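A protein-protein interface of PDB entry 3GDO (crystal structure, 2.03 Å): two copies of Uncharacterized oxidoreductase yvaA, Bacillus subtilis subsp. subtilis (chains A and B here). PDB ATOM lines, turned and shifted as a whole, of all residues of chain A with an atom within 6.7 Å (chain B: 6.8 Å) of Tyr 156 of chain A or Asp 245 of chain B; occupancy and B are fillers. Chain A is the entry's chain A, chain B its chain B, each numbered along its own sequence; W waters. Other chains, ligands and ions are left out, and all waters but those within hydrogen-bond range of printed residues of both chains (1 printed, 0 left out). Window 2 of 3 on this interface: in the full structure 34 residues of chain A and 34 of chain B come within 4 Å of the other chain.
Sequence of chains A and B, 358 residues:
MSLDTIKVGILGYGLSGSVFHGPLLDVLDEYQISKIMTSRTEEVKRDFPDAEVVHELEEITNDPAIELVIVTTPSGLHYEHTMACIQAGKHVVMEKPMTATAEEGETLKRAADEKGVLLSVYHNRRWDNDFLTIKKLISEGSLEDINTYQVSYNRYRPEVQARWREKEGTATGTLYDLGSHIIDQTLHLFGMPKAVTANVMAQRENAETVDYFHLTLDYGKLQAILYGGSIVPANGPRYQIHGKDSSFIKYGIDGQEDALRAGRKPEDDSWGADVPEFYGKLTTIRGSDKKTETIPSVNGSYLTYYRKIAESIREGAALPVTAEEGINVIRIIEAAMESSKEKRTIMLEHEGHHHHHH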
ATOM      1  N   ASN A 154     -24.653  -8.008 -16.953  1.00  0.00           N
ATOM      2  CA  ASN A 154     -23.211  -8.143 -17.227  1.00  0.00           C
ATOM      3  C   ASN A 154     -22.789  -9.583 -17.425  1.00  0.00           C
ATOM      4  O   ASN A 154     -23.499 -10.491 -17.031  1.00  0.00           O
ATOM      5  CB  ASN A 154     -22.401  -7.632 -16.042  1.00  0.00           C
ATOM      6  CG  ASN A 154     -22.554  -6.158 -15.843  1.00  0.00           C
ATOM      7  OD1 ASN A 154     -22.509  -5.384 -16.796  1.00  0.00           O
ATOM      8  ND2 ASN A 154     -22.721  -5.752 -14.601  1.00  0.00           N
ATOM      9  N   ARG A 155     -21.614  -9.793 -18.000  1.00  0.00           N
ATOM     10  CA  ARG A 155     -21.053 -11.137 -18.042  1.00  0.00           C
ATOM     11  C   ARG A 155     -19.542 -10.987 -18.118  1.00  0.00           C
ATOM     12  O   ARG A 155     -19.025  -9.892 -18.393  1.00  0.00           O
ATOM     13  CB  ARG A 155     -21.647 -11.962 -19.202  1.00  0.00           C
ATOM     14  CG  ARG A 155     -21.102 -11.628 -20.539  1.00  0.00           C
ATOM     15  CD  ARG A 155     -22.172 -11.469 -21.616  1.00  0.00           C
ATOM     16  NE  ARG A 155     -21.518 -10.965 -22.815  1.00  0.00           N
ATOM     17  CZ  ARG A 155     -21.495 -11.589 -23.987  1.00  0.00           C
ATOM     18  NH1 ARG A 155     -20.836 -11.036 -25.003  1.00  0.00           N
ATOM     19  NH2 ARG A 155     -22.157 -12.738 -24.152  1.00  0.00           N
ATOM     20  N   TYR A 156     -18.845 -12.063 -17.792  1.00  0.00           N
ATOM     21  CA  TYR A 156     -17.401 -12.073 -17.917  1.00  0.00           C
ATOM     22  C   TYR A 156     -17.045 -12.977 -19.091  1.00  0.00           C
ATOM     23  O   TYR A 156     -16.937 -14.185 -18.919  1.00  0.00           O
ATOM     24  CB  TYR A 156     -16.753 -12.572 -16.632  1.00  0.00           C
ATOM     25  CG  TYR A 156     -15.254 -12.427 -16.687  1.00  0.00           C
ATOM     26  CD1 TYR A 156     -14.668 -11.155 -16.820  1.00  0.00           C
ATOM     27  CD2 TYR A 156     -14.407 -13.559 -16.666  1.00  0.00           C
ATOM     28  CE1 TYR A 156     -13.309 -11.002 -16.902  1.00  0.00           C
ATOM     29  CE2 TYR A 156     -13.002 -13.412 -16.749  1.00  0.00           C
ATOM     30  CZ  TYR A 156     -12.461 -12.128 -16.849  1.00  0.00           C
ATOM     31  OH  TYR A 156     -11.082 -11.928 -16.924  1.00  0.00           O
ATOM     32  N   ARG A 157     -16.919 -12.394 -20.277  1.00  0.00           N
ATOM     33  CA  ARG A 157     -16.533 -13.129 -21.479  1.00  0.00           C
ATOM     34  C   ARG A 157     -15.394 -12.399 -22.144  1.00  0.00           C
ATOM     35  O   ARG A 157     -15.573 -11.890 -23.260  1.00  0.00           O
ATOM     36  CB  ARG A 157     -17.672 -13.166 -22.501  1.00  0.00           C
ATOM     37  CG  ARG A 157     -18.645 -14.306 -22.386  1.00  0.00           C
ATOM     38  CD  ARG A 157     -19.121 -14.697 -23.801  1.00  0.00           C
ATOM     39  NE  ARG A 157     -20.338 -15.527 -23.886  1.00  0.00           N
ATOM     40  CZ  ARG A 157     -21.046 -16.029 -22.869  1.00  0.00           C
ATOM     41  NH1 ARG A 157     -20.696 -15.834 -21.594  1.00  0.00           N
ATOM     42  NH2 ARG A 157     -22.125 -16.754 -23.139  1.00  0.00           N
ATOM     43  N   PRO A 158     -14.222 -12.350 -21.493  1.00  0.00           N
ATOM     44  CA  PRO A 158     -13.126 -11.489 -21.975  1.00  0.00           C
ATOM     45  C   PRO A 158     -12.645 -11.854 -23.379  1.00  0.00           C
ATOM     46  O   PRO A 158     -12.296 -10.963 -24.159  1.00  0.00           O
ATOM     47  CB  PRO A 158     -12.028 -11.701 -20.943  1.00  0.00           C
ATOM     48  CG  PRO A 158     -12.308 -13.051 -20.351  1.00  0.00           C
ATOM     49  CD  PRO A 158     -13.814 -13.208 -20.372  1.00  0.00           C
ATOM     50  N   GLU A 159     -12.662 -13.148 -23.706  1.00  0.00           N
ATOM     51  CA  GLU A 159     -12.354 -13.613 -25.071  1.00  0.00           C
ATOM     52  C   GLU A 159     -13.575 -13.660 -25.977  1.00  0.00           C
ATOM     53  O   GLU A 159     -14.598 -14.234 -25.628  1.00  0.00           O
ATOM     54  CB  GLU A 159     -11.651 -14.981 -25.065  1.00  0.00           C
ATOM     55  CG  GLU A 159     -10.211 -14.903 -25.592  1.00  0.00           C
ATOM     56  CD  GLU A 159      -9.436 -13.755 -24.946  1.00  0.00           C
ATOM     57  OE1 GLU A 159      -9.063 -12.790 -25.660  1.00  0.00           O
ATOM     58  OE2 GLU A 159      -9.235 -13.799 -23.708  1.00  0.00           O
ATOM     59  N   GLY A 229     -22.019  -4.932 -19.547  1.00  0.00           N
ATOM     60  CA  GLY A 229     -20.731  -5.097 -20.221  1.00  0.00           C
ATOM     61  C   GLY A 229     -20.352  -6.580 -20.280  1.00  0.00           C
ATOM     62  O   GLY A 229     -20.991  -7.417 -19.627  1.00  0.00           O
ATOM     63  N   SER A 230     -19.319  -6.899 -21.062  1.00  0.00           N
ATOM     64  CA  SER A 230     -18.793  -8.261 -21.198  1.00  0.00           C
ATOM     65  C   SER A 230     -17.401  -8.477 -20.589  1.00  0.00           C
ATOM     66  O   SER A 230     -16.809  -9.562 -20.766  1.00  0.00           O
ATOM     67  CB  SER A 230     -18.749  -8.637 -22.673  1.00  0.00           C
ATOM     68  OG  SER A 230     -20.002  -8.368 -23.243  1.00  0.00           O
ATOM     69  N   ILE A 231     -16.865  -7.474 -19.878  1.00  0.00           N
ATOM     70  CA  ILE A 231     -15.647  -7.693 -19.087  1.00  0.00           C
ATOM     71  C   ILE A 231     -15.887  -7.343 -17.637  1.00  0.00           C
ATOM     72  O   ILE A 231     -15.277  -6.413 -17.098  1.00  0.00           O
ATOM     73  CB  ILE A 231     -14.426  -6.913 -19.613  1.00  0.00           C
ATOM     74  CG1 ILE A 231     -14.386  -6.957 -21.139  1.00  0.00           C
ATOM     75  CG2 ILE A 231     -13.132  -7.445 -18.941  1.00  0.00           C
ATOM     76  CD1 ILE A 231     -13.553  -5.852 -21.757  1.00  0.00           C
ATOM     77  N   VAL A 232     -16.799  -8.083 -17.017  1.00  0.00           N
ATOM     78  CA  VAL A 232     -17.237  -7.793 -15.651  1.00  0.00           C
ATOM     79  C   VAL A 232     -17.092  -9.029 -14.761  1.00  0.00           C
ATOM     80  O   VAL A 232     -17.979  -9.884 -14.743  1.00  0.00           O
ATOM     81  CB  VAL A 232     -18.712  -7.319 -15.640  1.00  0.00           C
ATOM     82  CG1 VAL A 232     -19.221  -7.144 -14.204  1.00  0.00           C
ATOM     83  CG2 VAL A 232     -18.890  -6.035 -16.487  1.00  0.00           C
ATOM     84  N   PRO A 233     -15.970  -9.139 -14.025  1.00  0.00           N
ATOM     85  CA  PRO A 233     -15.750 -10.284 -13.101  1.00  0.00           C
ATOM     86  C   PRO A 233     -16.793 -10.477 -11.983  1.00  0.00           C
ATOM     87  O   PRO A 233     -17.207 -11.622 -11.723  1.00  0.00           O
ATOM     88  CB  PRO A 233     -14.347  -9.993 -12.508  1.00  0.00           C
ATOM     89  CG  PRO A 233     -13.672  -9.200 -13.555  1.00  0.00           C
ATOM     90  CD  PRO A 233     -14.731  -8.366 -14.235  1.00  0.00           C
ATOM     91  N   ALA A 234     -17.208  -9.402 -11.294  1.00  0.00           N
ATOM     92  CA  ALA A 234     -18.307  -9.502 -10.312  1.00  0.00           C
ATOM     93  C   ALA A 234     -19.361  -8.444 -10.575  1.00  0.00           C
ATOM     94  O   ALA A 234     -19.061  -7.264 -10.757  1.00  0.00           O
ATOM     95  CB  ALA A 234     -17.807  -9.403  -8.855  1.00  0.00           C
ATOM     96  N   ASN A 235     -20.603  -8.882 -10.618  1.00  0.00           N
ATOM     97  CA  ASN A 235     -21.705  -7.982 -10.909  1.00  0.00           C
ATOM     98  C   ASN A 235     -22.085  -7.211  -9.660  1.00  0.00           C
ATOM     99  O   ASN A 235     -21.902  -7.651  -8.514  1.00  0.00           O
ATOM    100  CB  ASN A 235     -22.884  -8.776 -11.472  1.00  0.00           C
ATOM    101  CG  ASN A 235     -22.474  -9.643 -12.624  1.00  0.00           C
ATOM    102  OD1 ASN A 235     -21.939  -9.152 -13.610  1.00  0.00           O
ATOM    103  ND2 ASN A 235     -22.688 -10.951 -12.503  1.00  0.00           N
ATOM    104  N   SER B 142      -3.752  -5.076  -8.531  1.00  0.00           N
ATOM    105  CA  SER B 142      -4.925  -5.935  -8.293  1.00  0.00           C
ATOM    106  C   SER B 142      -6.181  -5.423  -9.018  1.00  0.00           C
ATOM    107  O   SER B 142      -7.272  -5.998  -8.870  1.00  0.00           O
ATOM    108  CB  SER B 142      -5.198  -6.083  -6.790  1.00  0.00           C
ATOM    109  OG  SER B 142      -4.014  -6.443  -6.077  1.00  0.00           O
ATOM    110  N   GLU B 144      -6.021  -4.099 -12.706  1.00  0.00           N
ATOM    111  CA  GLU B 144      -5.464  -3.755 -14.031  1.00  0.00           C
ATOM    112  C   GLU B 144      -6.476  -3.493 -15.149  1.00  0.00           C
ATOM    113  O   GLU B 144      -7.535  -4.153 -15.216  1.00  0.00           O
ATOM    114  CB  GLU B 144      -4.525  -4.875 -14.496  1.00  0.00           C
ATOM    115  CG  GLU B 144      -3.315  -5.097 -13.578  1.00  0.00           C
ATOM    116  CD  GLU B 144      -2.228  -4.039 -13.791  1.00  0.00           C
ATOM    117  OE1 GLU B 144      -1.737  -3.902 -14.941  1.00  0.00           O
ATOM    118  OE2 GLU B 144      -1.868  -3.343 -12.806  1.00  0.00           O
ATOM    119  N   ASP B 145      -6.121  -2.547 -16.031  1.00  0.00           N
ATOM    120  CA  ASP B 145      -6.863  -2.256 -17.248  1.00  0.00           C
ATOM    121  C   ASP B 145      -8.350  -2.117 -16.890  1.00  0.00           C
ATOM    122  O   ASP B 145      -9.175  -2.953 -17.262  1.00  0.00           O
ATOM    123  CB  ASP B 145      -6.636  -3.346 -18.304  1.00  0.00           C
ATOM    124  CG  ASP B 145      -7.262  -2.993 -19.679  1.00  0.00           C
ATOM    125  OD1 ASP B 145      -7.299  -1.797 -20.060  1.00  0.00           O
ATOM    126  OD2 ASP B 145      -7.730  -3.917 -20.399  1.00  0.00           O
ATOM    127  N   ASN B 147     -11.976  -1.122 -17.095  1.00  0.00           N
ATOM    128  CA  ASN B 147     -12.796  -0.847 -18.276  1.00  0.00           C
ATOM    129  C   ASN B 147     -14.096  -0.104 -17.925  1.00  0.00           C
ATOM    130  O   ASN B 147     -14.690   0.548 -18.769  1.00  0.00           O
ATOM    131  CB  ASN B 147     -13.069  -2.142 -19.072  1.00  0.00           C
ATOM    132  CG  ASN B 147     -13.870  -3.167 -18.284  1.00  0.00           C
ATOM    133  OD1 ASN B 147     -15.060  -2.958 -17.986  1.00  0.00           O
ATOM    134  ND2 ASN B 147     -13.239  -4.277 -17.948  1.00  0.00           N
ATOM    135  N   HIS B 242     -14.591  -2.420 -12.662  1.00  0.00           N
ATOM    136  CA  HIS B 242     -14.303  -3.651 -13.412  1.00  0.00           C
ATOM    137  C   HIS B 242     -13.085  -3.484 -14.293  1.00  0.00           C
ATOM    138  O   HIS B 242     -13.033  -2.555 -15.134  1.00  0.00           O
ATOM    139  CB  HIS B 242     -15.504  -4.076 -14.279  1.00  0.00           C
ATOM    140  CG  HIS B 242     -16.799  -4.057 -13.533  1.00  0.00           C
ATOM    141  ND1 HIS B 242     -16.986  -4.774 -12.371  1.00  0.00           N
ATOM    142  CD2 HIS B 242     -17.972  -3.406 -13.777  1.00  0.00           C
ATOM    143  CE1 HIS B 242     -18.203  -4.532 -11.902  1.00  0.00           C
ATOM    144  NE2 HIS B 242     -18.817  -3.694 -12.727  1.00  0.00           N
ATOM    145  N   GLY B 243     -12.115  -4.378 -14.106  1.00  0.00           N
ATOM    146  CA  GLY B 243     -10.900  -4.433 -14.949  1.00  0.00           C
ATOM    147  C   GLY B 243     -10.748  -5.755 -15.699  1.00  0.00           C
ATOM    148  O   GLY B 243     -11.664  -6.590 -15.679  1.00  0.00           O
ATOM    149  N   LYS B 244      -9.594  -5.995 -16.331  1.00  0.00           N
ATOM    150  CA  LYS B 244      -9.457  -7.239 -17.140  1.00  0.00           C
ATOM    151  C   LYS B 244      -9.711  -8.546 -16.387  1.00  0.00           C
ATOM    152  O   LYS B 244     -10.269  -9.472 -16.965  1.00  0.00           O
ATOM    153  CB  LYS B 244      -8.158  -7.300 -17.985  1.00  0.00           C
ATOM    154  CG  LYS B 244      -6.819  -7.368 -17.237  1.00  0.00           C
ATOM    155  CD  LYS B 244      -5.810  -8.155 -18.094  1.00  0.00           C
ATOM    156  CE  LYS B 244      -4.334  -7.750 -17.905  1.00  0.00           C
ATOM    157  NZ  LYS B 244      -3.926  -7.651 -16.477  1.00  0.00           N
ATOM    158  N   ASP B 245      -9.408  -8.567 -15.087  1.00  0.00           N
ATOM    159  CA  ASP B 245      -9.262  -9.786 -14.265  1.00  0.00           C
ATOM    160  C   ASP B 245     -10.019  -9.744 -12.969  1.00  0.00           C
ATOM    161  O   ASP B 245     -10.170 -10.765 -12.285  1.00  0.00           O
ATOM    162  CB  ASP B 245      -7.792  -9.889 -13.821  1.00  0.00           C
ATOM    163  CG  ASP B 245      -6.968 -10.689 -14.772  1.00  0.00           C
ATOM    164  OD1 ASP B 245      -5.824 -11.061 -14.408  1.00  0.00           O
ATOM    165  OD2 ASP B 245      -7.491 -10.971 -15.887  1.00  0.00           O
ATOM    166  N   SER B 246     -10.400  -8.535 -12.572  1.00  0.00           N
ATOM    167  CA  SER B 246     -10.939  -8.296 -11.250  1.00  0.00           C
ATOM    168  C   SER B 246     -11.977  -7.174 -11.239  1.00  0.00           C
ATOM    169  O   SER B 246     -12.032  -6.350 -12.162  1.00  0.00           O
ATOM    170  CB  SER B 246      -9.795  -7.969 -10.294  1.00  0.00           C
ATOM    171  OG  SER B 246      -8.997  -6.943 -10.850  1.00  0.00           O
ATOM    172  N   SER B 247     -12.783  -7.187 -10.183  1.00  0.00           N
ATOM    173  CA  SER B 247     -13.845  -6.229  -9.888  1.00  0.00           C
ATOM    174  C   SER B 247     -13.727  -5.859  -8.420  1.00  0.00           C
ATOM    175  O   SER B 247     -13.466  -6.748  -7.554  1.00  0.00           O
ATOM    176  CB  SER B 247     -15.213  -6.881 -10.054  1.00  0.00           C
ATOM    177  OG  SER B 247     -15.595  -7.024 -11.398  1.00  0.00           O
ATOM    178  N   THR B 283     -13.047  -9.270  -6.330  1.00  0.00           N
ATOM    179  CA  THR B 283     -13.208 -10.549  -7.004  1.00  0.00           C
ATOM    180  C   THR B 283     -12.154 -10.640  -8.091  1.00  0.00           C
ATOM    181  O   THR B 283     -12.031  -9.714  -8.899  1.00  0.00           O
ATOM    182  CB  THR B 283     -14.588 -10.653  -7.591  1.00  0.00           C
ATOM    183  OG1 THR B 283     -15.522 -10.646  -6.514  1.00  0.00           O
ATOM    184  CG2 THR B 283     -14.757 -11.940  -8.383  1.00  0.00           C
ATOM    185  N   THR B 284     -11.375 -11.732  -8.061  1.00  0.00           N
ATOM    186  CA  THR B 284     -10.324 -11.990  -9.052  1.00  0.00           C
ATOM    187  C   THR B 284     -10.527 -13.316  -9.802  1.00  0.00           C
ATOM    188  O   THR B 284     -10.812 -14.350  -9.191  1.00  0.00           O
ATOM    189  CB  THR B 284      -8.909 -11.940  -8.406  1.00  0.00           C
ATOM    190  OG1 THR B 284      -8.764 -10.710  -7.684  1.00  0.00           O
ATOM    191  CG2 THR B 284      -7.833 -12.023  -9.465  1.00  0.00           C
ATOM    192  N   ILE B 285     -10.391 -13.261 -11.121  1.00  0.00           N
ATOM    193  CA  ILE B 285     -10.489 -14.453 -11.950  1.00  0.00           C
ATOM    194  C   ILE B 285      -9.198 -14.751 -12.716  1.00  0.00           C
ATOM    195  O   ILE B 285      -8.808 -13.997 -13.617  1.00  0.00           O
ATOM    196  CB  ILE B 285     -11.700 -14.430 -12.951  1.00  0.00           C
ATOM    197  CG1 ILE B 285     -12.972 -13.892 -12.263  1.00  0.00           C
ATOM    198  CG2 ILE B 285     -11.919 -15.840 -13.556  1.00  0.00           C
ATOM    199  CD1 ILE B 285     -14.320 -14.273 -12.898  1.00  0.00           C
ATOM    200  N   ARG B 286      -8.561 -15.863 -12.346  1.00  0.00           N
ATOM    201  CA  ARG B 286      -7.442 -16.455 -13.103  1.00  0.00           C
ATOM    202  C   ARG B 286      -7.949 -17.740 -13.768  1.00  0.00           C
ATOM    203  O   ARG B 286      -8.254 -18.734 -13.087  1.00  0.00           O
ATOM    204  CB  ARG B 286      -6.239 -16.752 -12.184  1.00  0.00           C
ATOM    205  N   GLY B 287      -8.078 -17.696 -15.093  1.00  0.00           N
ATOM    206  CA  GLY B 287      -8.594 -18.826 -15.862  1.00  0.00           C
ATOM    207  C   GLY B 287      -9.986 -19.288 -15.460  1.00  0.00           C
ATOM    208  O   GLY B 287     -10.991 -18.663 -15.809  1.00  0.00           O
HETATM  209  O   HOH W   1     -17.125  -4.570 -19.379  1.00  0.00           O
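Water W1 lies within hydrogen-bond range of N of Ile 231 of chain A (3.0 Å) and OD1 of Asn 147 of chain B (3.0 Å).
Of chain B, only Lys 244, Asp 245 and Ile 285 come within 4 Å of Tyr 156 of chain A.
Of the printed residues of chain A, Asp 245 of chain B touches Tyr 156 and Pro 233.
Printed residues of chain A within 4 Å of Ser 247 of chain B: Pro 233 and Ala 234.
Of the printed residues of chain A, Ile 285 of chain B touches Tyr 156 (3.8 Å).
The nearest residue of chain A that does not touch Asp 245 of chain B is Ile 231 of chain A (5.5 Å).
The nearest printed residue of chain A that does not touch Lys 244 of chain B is Ile 231 of chain A (4.03 Å).
Tyr 156 of chain A touches Asp 245 of chain B (OH to OD2, 3.9 Å).
Tyr 156 of chain A touches Ile 285 of chain B (CD2 to CD1, 3.8 Å).
His 242 of chain B touches Ile 231 of chain A.
O of Gly 243 of chain B touches CG2 of Ile 231 of chain A, at 3.7 Å.
His 242 of chain B touches Val 232 of chain A.
Pro 233 of chain A touches Gly 243 of chain B (CD to O, 3.8 Å).
Pro 233 of chain A touches Asp 245 of chain B.
N of Ser 246 of chain B touches CG of Pro 233 of chain A, at 3.5 Å.
O of Ala 234 of chain A touches CE1 of His 242 of chain B, 3.1 Å away.
CB of Ala 234 of chain A touches OG1 of Thr 283 of chain B, 3.5 Å away.
O of Lys 244 of chain B sits at hydrogen-bond distance from OH of Tyr 156 of chain A, at 2.6 Å.
The side-chain amide nitrogen (ND2) of Asn 147 of chain B sits at hydrogen-bond distance from the backbone carbonyl oxygen (O) of Ile 231 of chain A (3.1 Å).
The backbone nitrogen (N) of Pro 233 of chain A sits close to the side-chain hydroxyl (OG) of Ser 247 of chain B, 3.4 Å away.
The side-chain hydroxyl (OG) of Ser 247 of chain B lies within hydrogen-bond range of the backbone NH (N) of Ala 234 of chain A.
A ring nitrogen (ND1) of His 242 of chain B sits at hydrogen-bond distance from the side-chain hydroxyl (OG) of Ser 247 of chain B, 2.8 Å away.
The backbone carbonyl oxygen of Arg 155 of chain A lies within hydrogen-bond range of the backbone NH of Val 232 of chain A.
The backbone NH of Thr 283 of chain B is in hydrogen-bond range of the backbone carbonyl oxygen of Ser 247 of chain B.
The backbone NH of Asn 147 of chain B is in hydrogen-bond range of the backbone carbonyl oxygen of His 242 of chain B, 2.6 Å away.
The backbone carbonyl oxygen (O) of Glu 144 of chain B is in hydrogen-bond range of the backbone NH (N) of Lys 244 of chain B, at 3.0 Å.
O of Asp 145 of chain B sits at hydrogen-bond distance from N of Lys 244 of chain B, 3.2 Å away.
Printed residues of chain A that touch a printed residue of chain B: Tyr 156, Ile 231, Val 232, Pro 233 and Ala 234.
Printed residues of chain B that touch a printed residue of chain A: Asn 147, His 242, Gly 243, Lys 244, Asp 245, Ser 246, Ser 247, Thr 283 and Ile 285.
Among the printed residues, no Asp or Glu carboxylate lies within 4 Å of a Lys or Arg side-chain nitrogen of the other chain.
No position is printed for both chains.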
